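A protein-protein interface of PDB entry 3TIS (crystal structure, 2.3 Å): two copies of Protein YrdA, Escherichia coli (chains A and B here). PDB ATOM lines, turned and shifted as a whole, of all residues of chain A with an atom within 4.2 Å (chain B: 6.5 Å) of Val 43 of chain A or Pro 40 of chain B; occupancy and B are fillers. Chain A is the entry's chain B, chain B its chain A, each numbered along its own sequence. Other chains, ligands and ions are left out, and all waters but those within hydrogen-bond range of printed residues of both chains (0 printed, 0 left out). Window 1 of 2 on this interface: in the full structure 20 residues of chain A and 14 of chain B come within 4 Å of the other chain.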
ATOM      1  N   VAL A  25     -31.659  23.247 -26.888  1.00  0.00           N
ATOM      2  CA  VAL A  25     -30.268  23.670 -26.934  1.00  0.00           C
ATOM      3  C   VAL A  25     -29.557  23.122 -28.171  1.00  0.00           C
ATOM      4  O   VAL A  25     -29.588  21.920 -28.433  1.00  0.00           O
ATOM      5  CB  VAL A  25     -29.555  23.183 -25.658  1.00  0.00           C
ATOM      6  CG1 VAL A  25     -28.157  23.763 -25.558  1.00  0.00           C
ATOM      7  CG2 VAL A  25     -30.375  23.576 -24.449  1.00  0.00           C
ATOM      8  N   VAL A  42     -35.049  19.579 -26.521  1.00  0.00           N
ATOM      9  CA  VAL A  42     -34.190  18.754 -27.345  1.00  0.00           C
ATOM     10  C   VAL A  42     -32.783  19.330 -27.252  1.00  0.00           C
ATOM     11  O   VAL A  42     -32.616  20.542 -27.145  1.00  0.00           O
ATOM     12  CB  VAL A  42     -34.654  18.775 -28.814  1.00  0.00           C
ATOM     13  CG1 VAL A  42     -33.648  18.027 -29.697  1.00  0.00           C
ATOM     14  CG2 VAL A  42     -36.055  18.150 -28.921  1.00  0.00           C
ATOM     15  N   VAL A  43     -31.776  18.463 -27.268  1.00  0.00           N
ATOM     16  CA  VAL A  43     -30.391  18.907 -27.223  1.00  0.00           C
ATOM     17  C   VAL A  43     -29.640  18.326 -28.411  1.00  0.00           C
ATOM     18  O   VAL A  43     -29.692  17.122 -28.660  1.00  0.00           O
ATOM     19  CB  VAL A  43     -29.663  18.455 -25.927  1.00  0.00           C
ATOM     20  CG1 VAL A  43     -28.198  18.870 -25.992  1.00  0.00           C
ATOM     21  CG2 VAL A  43     -30.314  19.089 -24.698  1.00  0.00           C
ATOM     22  N   ILE A  44     -28.954  19.193 -29.149  1.00  0.00           N
ATOM     23  CA  ILE A  44     -28.167  18.791 -30.304  1.00  0.00           C
ATOM     24  C   ILE A  44     -26.779  19.383 -30.072  1.00  0.00           C
ATOM     25  O   ILE A  44     -26.581  20.591 -30.179  1.00  0.00           O
ATOM     26  CB  ILE A  44     -28.755  19.350 -31.620  1.00  0.00           C
ATOM     27  CG1 ILE A  44     -30.223  18.948 -31.748  1.00  0.00           C
ATOM     28  CG2 ILE A  44     -27.978  18.810 -32.807  1.00  0.00           C
ATOM     29  CD1 ILE A  44     -30.901  19.487 -33.002  1.00  0.00           C
ATOM     30  N   ARG A  45     -25.823  18.526 -29.746  1.00  0.00           N
ATOM     31  CA  ARG A  45     -24.478  18.980 -29.458  1.00  0.00           C
ATOM     32  C   ARG A  45     -23.464  18.488 -30.471  1.00  0.00           C
ATOM     33  O   ARG A  45     -22.995  17.357 -30.396  1.00  0.00           O
ATOM     34  CB  ARG A  45     -24.088  18.526 -28.047  1.00  0.00           C
ATOM     35  CG  ARG A  45     -22.713  18.956 -27.603  1.00  0.00           C
ATOM     36  CD  ARG A  45     -22.668  19.130 -26.092  1.00  0.00           C
ATOM     37  NE  ARG A  45     -22.937  17.898 -25.355  1.00  0.00           N
ATOM     38  CZ  ARG A  45     -22.008  17.020 -24.980  1.00  0.00           C
ATOM     39  NH1 ARG A  45     -20.734  17.227 -25.273  1.00  0.00           N
ATOM     40  NH2 ARG A  45     -22.351  15.944 -24.285  1.00  0.00           N
ATOM     41  N   SER A  63     -35.649  14.668 -27.603  1.00  0.00           N
ATOM     42  CA  SER A  63     -34.600  13.928 -28.296  1.00  0.00           C
ATOM     43  C   SER A  63     -33.218  14.431 -27.873  1.00  0.00           C
ATOM     44  O   SER A  63     -33.062  15.568 -27.410  1.00  0.00           O
ATOM     45  CB  SER A  63     -34.759  14.062 -29.813  1.00  0.00           C
ATOM     46  OG  SER A  63     -35.855  13.289 -30.271  1.00  0.00           O
ATOM     47  N   MET A  64     -32.216  13.576 -28.043  1.00  0.00           N
ATOM     48  CA  MET A  64     -30.853  13.924 -27.668  1.00  0.00           C
ATOM     49  C   MET A  64     -29.910  13.481 -28.788  1.00  0.00           C
ATOM     50  O   MET A  64     -29.867  12.307 -29.144  1.00  0.00           O
ATOM     51  CB  MET A  64     -30.511  13.228 -26.344  1.00  0.00           C
ATOM     52  CG  MET A  64     -29.406  13.888 -25.538  1.00  0.00           C
ATOM     53  SD  MET A  64     -27.773  13.813 -26.333  1.00  0.00           S
ATOM     54  CE  MET A  64     -27.390  15.590 -26.482  1.00  0.00           C
ATOM     55  N   LEU A  65     -29.170  14.429 -29.356  1.00  0.00           N
ATOM     56  CA  LEU A  65     -28.248  14.114 -30.449  1.00  0.00           C
ATOM     57  C   LEU A  65     -26.807  14.499 -30.147  1.00  0.00           C
ATOM     58  O   LEU A  65     -26.515  15.644 -29.798  1.00  0.00           O
ATOM     59  CB  LEU A  65     -28.677  14.816 -31.748  1.00  0.00           C
ATOM     60  CG  LEU A  65     -29.906  14.305 -32.492  1.00  0.00           C
ATOM     61  CD1 LEU A  65     -31.149  14.429 -31.617  1.00  0.00           C
ATOM     62  CD2 LEU A  65     -30.081  15.119 -33.764  1.00  0.00           C
ATOM     63  N   MET B  19     -19.197  22.917 -13.812  1.00  0.00           N
ATOM     64  CA  MET B  19     -20.051  23.466 -14.855  1.00  0.00           C
ATOM     65  C   MET B  19     -21.472  22.940 -14.766  1.00  0.00           C
ATOM     66  O   MET B  19     -21.695  21.747 -14.555  1.00  0.00           O
ATOM     67  CB  MET B  19     -19.521  23.137 -16.251  1.00  0.00           C
ATOM     68  CG  MET B  19     -20.492  23.562 -17.349  1.00  0.00           C
ATOM     69  SD  MET B  19     -20.215  22.786 -18.959  1.00  0.00           S
ATOM     70  CE  MET B  19     -21.105  21.223 -18.723  1.00  0.00           C
ATOM     71  N   ASP B  21     -24.896  23.584 -17.110  1.00  0.00           N
ATOM     72  CA  ASP B  21     -25.531  24.224 -18.258  1.00  0.00           C
ATOM     73  C   ASP B  21     -26.709  25.067 -17.777  1.00  0.00           C
ATOM     74  O   ASP B  21     -27.398  24.692 -16.829  1.00  0.00           O
ATOM     75  CB  ASP B  21     -26.034  23.168 -19.247  1.00  0.00           C
ATOM     76  CG  ASP B  21     -26.304  23.745 -20.635  1.00  0.00           C
ATOM     77  OD1 ASP B  21     -25.332  23.955 -21.393  1.00  0.00           O
ATOM     78  OD2 ASP B  21     -27.485  23.992 -20.962  1.00  0.00           O
ATOM     79  N   ASP B  22     -26.938  26.202 -18.430  1.00  0.00           N
ATOM     80  CA  ASP B  22     -28.038  27.087 -18.060  1.00  0.00           C
ATOM     81  C   ASP B  22     -29.405  26.439 -18.249  1.00  0.00           C
ATOM     82  O   ASP B  22     -30.394  26.887 -17.663  1.00  0.00           O
ATOM     83  CB  ASP B  22     -27.997  28.373 -18.885  1.00  0.00           C
ATOM     84  CG  ASP B  22     -26.745  29.180 -18.648  1.00  0.00           C
ATOM     85  OD1 ASP B  22     -26.406  29.438 -17.470  1.00  0.00           O
ATOM     86  OD2 ASP B  22     -26.106  29.566 -19.648  1.00  0.00           O
ATOM     87  N   SER B  23     -29.469  25.398 -19.072  1.00  0.00           N
ATOM     88  CA  SER B  23     -30.741  24.725 -19.326  1.00  0.00           C
ATOM     89  C   SER B  23     -31.051  23.661 -18.284  1.00  0.00           C
ATOM     90  O   SER B  23     -32.163  23.137 -18.238  1.00  0.00           O
ATOM     91  CB  SER B  23     -30.727  24.064 -20.702  1.00  0.00           C
ATOM     92  OG  SER B  23     -29.902  22.914 -20.687  1.00  0.00           O
ATOM     93  N   SER B  24     -30.067  23.343 -17.449  1.00  0.00           N
ATOM     94  CA  SER B  24     -30.244  22.318 -16.434  1.00  0.00           C
ATOM     95  C   SER B  24     -30.852  22.813 -15.128  1.00  0.00           C
ATOM     96  O   SER B  24     -30.800  24.001 -14.818  1.00  0.00           O
ATOM     97  CB  SER B  24     -28.911  21.623 -16.176  1.00  0.00           C
ATOM     98  OG  SER B  24     -28.562  20.842 -17.304  1.00  0.00           O
ATOM     99  N   ILE B  38     -22.134  19.251 -15.270  1.00  0.00           N
ATOM    100  CA  ILE B  38     -23.554  18.986 -15.475  1.00  0.00           C
ATOM    101  C   ILE B  38     -23.942  19.542 -16.843  1.00  0.00           C
ATOM    102  O   ILE B  38     -23.983  20.758 -17.041  1.00  0.00           O
ATOM    103  CB  ILE B  38     -24.411  19.652 -14.373  1.00  0.00           C
ATOM    104  CG1 ILE B  38     -23.873  19.258 -12.993  1.00  0.00           C
ATOM    105  CG2 ILE B  38     -25.869  19.227 -14.508  1.00  0.00           C
ATOM    106  CD1 ILE B  38     -23.765  17.767 -12.769  1.00  0.00           C
ATOM    107  N   TRP B  39     -24.229  18.641 -17.780  1.00  0.00           N
ATOM    108  CA  TRP B  39     -24.574  19.028 -19.144  1.00  0.00           C
ATOM    109  C   TRP B  39     -26.039  19.429 -19.405  1.00  0.00           C
ATOM    110  O   TRP B  39     -26.890  19.320 -18.521  1.00  0.00           O
ATOM    111  CB  TRP B  39     -24.109  17.924 -20.101  1.00  0.00           C
ATOM    112  CG  TRP B  39     -22.599  17.753 -20.078  1.00  0.00           C
ATOM    113  CD1 TRP B  39     -21.861  17.070 -19.148  1.00  0.00           C
ATOM    114  CD2 TRP B  39     -21.650  18.347 -20.978  1.00  0.00           C
ATOM    115  NE1 TRP B  39     -20.517  17.208 -19.413  1.00  0.00           N
ATOM    116  CE2 TRP B  39     -20.360  17.986 -20.528  1.00  0.00           C
ATOM    117  CE3 TRP B  39     -21.766  19.151 -22.117  1.00  0.00           C
ATOM    118  CZ2 TRP B  39     -19.194  18.400 -21.179  1.00  0.00           C
ATOM    119  CZ3 TRP B  39     -20.611  19.562 -22.762  1.00  0.00           C
ATOM    120  CH2 TRP B  39     -19.340  19.184 -22.291  1.00  0.00           C
ATOM    121  N   PRO B  40     -26.344  19.917 -20.627  1.00  0.00           N
ATOM    122  CA  PRO B  40     -27.693  20.350 -21.015  1.00  0.00           C
ATOM    123  C   PRO B  40     -28.907  19.525 -20.628  1.00  0.00           C
ATOM    124  O   PRO B  40     -28.901  18.291 -20.685  1.00  0.00           O
ATOM    125  CB  PRO B  40     -27.581  20.517 -22.527  1.00  0.00           C
ATOM    126  CG  PRO B  40     -26.196  21.044 -22.682  1.00  0.00           C
ATOM    127  CD  PRO B  40     -25.397  20.150 -21.736  1.00  0.00           C
ATOM    128  N   LEU B  41     -29.951  20.258 -20.244  1.00  0.00           N
ATOM    129  CA  LEU B  41     -31.246  19.712 -19.863  1.00  0.00           C
ATOM    130  C   LEU B  41     -31.223  18.562 -18.868  1.00  0.00           C
ATOM    131  O   LEU B  41     -31.930  17.572 -19.038  1.00  0.00           O
ATOM    132  CB  LEU B  41     -32.013  19.307 -21.127  1.00  0.00           C
ATOM    133  CG  LEU B  41     -32.418  20.479 -22.035  1.00  0.00           C
ATOM    134  CD1 LEU B  41     -33.115  19.953 -23.290  1.00  0.00           C
ATOM    135  CD2 LEU B  41     -33.351  21.422 -21.274  1.00  0.00           C
ATOM    136  N   VAL B  42     -30.411  18.696 -17.826  1.00  0.00           N
ATOM    137  CA  VAL B  42     -30.331  17.674 -16.797  1.00  0.00           C
ATOM    138  C   VAL B  42     -31.112  18.143 -15.580  1.00  0.00           C
ATOM    139  O   VAL B  42     -31.225  19.335 -15.319  1.00  0.00           O
ATOM    140  CB  VAL B  42     -28.881  17.421 -16.332  1.00  0.00           C
ATOM    141  CG1 VAL B  42     -28.883  16.478 -15.120  1.00  0.00           C
ATOM    142  CG2 VAL B  42     -28.054  16.841 -17.467  1.00  0.00           C
ATOM    143  N   ILE B  59     -22.102  14.240 -15.783  1.00  0.00           N
ATOM    144  CA  ILE B  59     -23.506  13.860 -15.887  1.00  0.00           C
ATOM    145  C   ILE B  59     -23.988  14.414 -17.233  1.00  0.00           C
ATOM    146  O   ILE B  59     -24.312  15.600 -17.353  1.00  0.00           O
ATOM    147  CB  ILE B  59     -24.356  14.472 -14.744  1.00  0.00           C
ATOM    148  CG1 ILE B  59     -23.782  14.074 -13.383  1.00  0.00           C
ATOM    149  CG2 ILE B  59     -25.794  13.981 -14.844  1.00  0.00           C
ATOM    150  CD1 ILE B  59     -23.793  12.574 -13.097  1.00  0.00           C
ATOM    151  N   GLN B  60     -24.040  13.543 -18.237  1.00  0.00           N
ATOM    152  CA  GLN B  60     -24.427  13.926 -19.591  1.00  0.00           C
ATOM    153  C   GLN B  60     -25.887  14.303 -19.880  1.00  0.00           C
ATOM    154  O   GLN B  60     -26.820  13.902 -19.174  1.00  0.00           O
ATOM    155  CB  GLN B  60     -23.964  12.841 -20.562  1.00  0.00           C
ATOM    156  CG  GLN B  60     -22.447  12.738 -20.658  1.00  0.00           C
ATOM    157  CD  GLN B  60     -21.989  11.547 -21.485  1.00  0.00           C
ATOM    158  OE1 GLN B  60     -22.409  11.370 -22.630  1.00  0.00           O
ATOM    159  NE2 GLN B  60     -21.121  10.723 -20.905  1.00  0.00           N
ATOM    160  N   ASP B  61     -26.036  15.087 -20.950  1.00  0.00           N
ATOM    161  CA  ASP B  61     -27.298  15.636 -21.455  1.00  0.00           C
ATOM    162  C   ASP B  61     -28.541  14.800 -21.240  1.00  0.00           C
ATOM    163  O   ASP B  61     -28.553  13.602 -21.514  1.00  0.00           O
ATOM    164  CB  ASP B  61     -27.191  15.912 -22.959  1.00  0.00           C
ATOM    165  CG  ASP B  61     -25.824  16.425 -23.372  1.00  0.00           C
ATOM    166  OD1 ASP B  61     -24.813  15.727 -23.128  1.00  0.00           O
ATOM    167  OD2 ASP B  61     -25.764  17.525 -23.958  1.00  0.00           O
ATOM    168  N   GLY B  62     -29.596  15.455 -20.768  1.00  0.00           N
ATOM    169  CA  GLY B  62     -30.867  14.783 -20.557  1.00  0.00           C
ATOM    170  C   GLY B  62     -30.951  13.722 -19.476  1.00  0.00           C
ATOM    171  O   GLY B  62     -31.923  12.966 -19.426  1.00  0.00           O
ATOM    172  N   SER B  63     -29.948  13.648 -18.609  1.00  0.00           N
ATOM    173  CA  SER B  63     -29.993  12.661 -17.542  1.00  0.00           C
ATOM    174  C   SER B  63     -30.957  13.117 -16.452  1.00  0.00           C
ATOM    175  O   SER B  63     -31.238  14.310 -16.310  1.00  0.00           O
ATOM    176  CB  SER B  63     -28.601  12.431 -16.958  1.00  0.00           C
ATOM    177  OG  SER B  63     -27.776  11.808 -17.923  1.00  0.00           O
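NH2 of Arg 45 of chain A is in salt-bridge range of OD1 of Asp 61 of chain B, at 2.7 Å.
The side-chain hydroxyl (OG) of Ser 23 of chain B is in hydrogen-bond range of the side-chain carboxylate (OD2) of Asp 21 of chain B (2.7 Å). N of Leu 41 of chain B lies within hydrogen-bond range of OG of Ser 24 of chain B (3.3 Å). O of Val 42 of chain A lies within hydrogen-bond range of N of Val 25 of chain A (2.9 Å). The backbone NH of Ile 44 of chain A sits at hydrogen-bond distance from the backbone carbonyl oxygen of Val 25 of chain A, at 2.9 Å. The backbone NH (N) of Val 43 of chain A is in hydrogen-bond range of the backbone carbonyl oxygen (O) of Ser 63 of chain A. The backbone carbonyl oxygen (O) of Val 43 of chain A is in hydrogen-bond range of the backbone NH (N) of Leu 65 of chain A (2.8 Å).
Among the printed residues, merely in contact across the chains: Val 25 of chain A with Ser 23 of chain B, Val 42 of chain A with Leu 41 of chain B, Val 43 of chain A with Pro 40 of chain B, Val 43 of chain A with Leu 41 of chain B, Val 43 of chain A with Asp 61 of chain B, Arg 45 of chain A with Trp 39 of chain B and Met 64 of chain A with Asp 61 of chain B.
Printed residues of chain B within 4 Å of Val 25 of chain A: Ser 23. Of chain B, only Pro 40 (3.8 Å), Leu 41 (3.3 Å) and Asp 61 (3.4 Å) come within 4 Å of Val 43 of chain A. Printed residues of chain B within 4 Å of Arg 45 of chain A: Trp 39 and Asp 61. Of the printed residues of chain B, Met 64 of chain A touches Asp 61. Of the printed residues of chain A, Trp 39 of chain B touches Arg 45. Pro 40 of chain B touches one residue of chain A. Of the printed residues of chain A, Leu 41 of chain B touches Val 42 and Val 43. The nearest residue of chain B that does not touch Val 43 of chain A is Gly 62 of chain B (5.4 Å). The nearest printed residue of chain A that does not touch Leu 41 of chain B is Val 25 of chain A (4.4 Å).
Hydrophobic or aromatic side chains of chain B that line the printed part of chain A: Trp 39, Pro 40 and Leu 41. Of the 8 printed residues of chain A, 5 touch a printed residue of chain B. Hydrophobic or aromatic side chains of chain A within 4 Å of the printed part of chain B: Val 25, Val 43 and Met 64. Among the printed residues, 8 pairs touch across the chains.
2 positions are printed for both chains.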
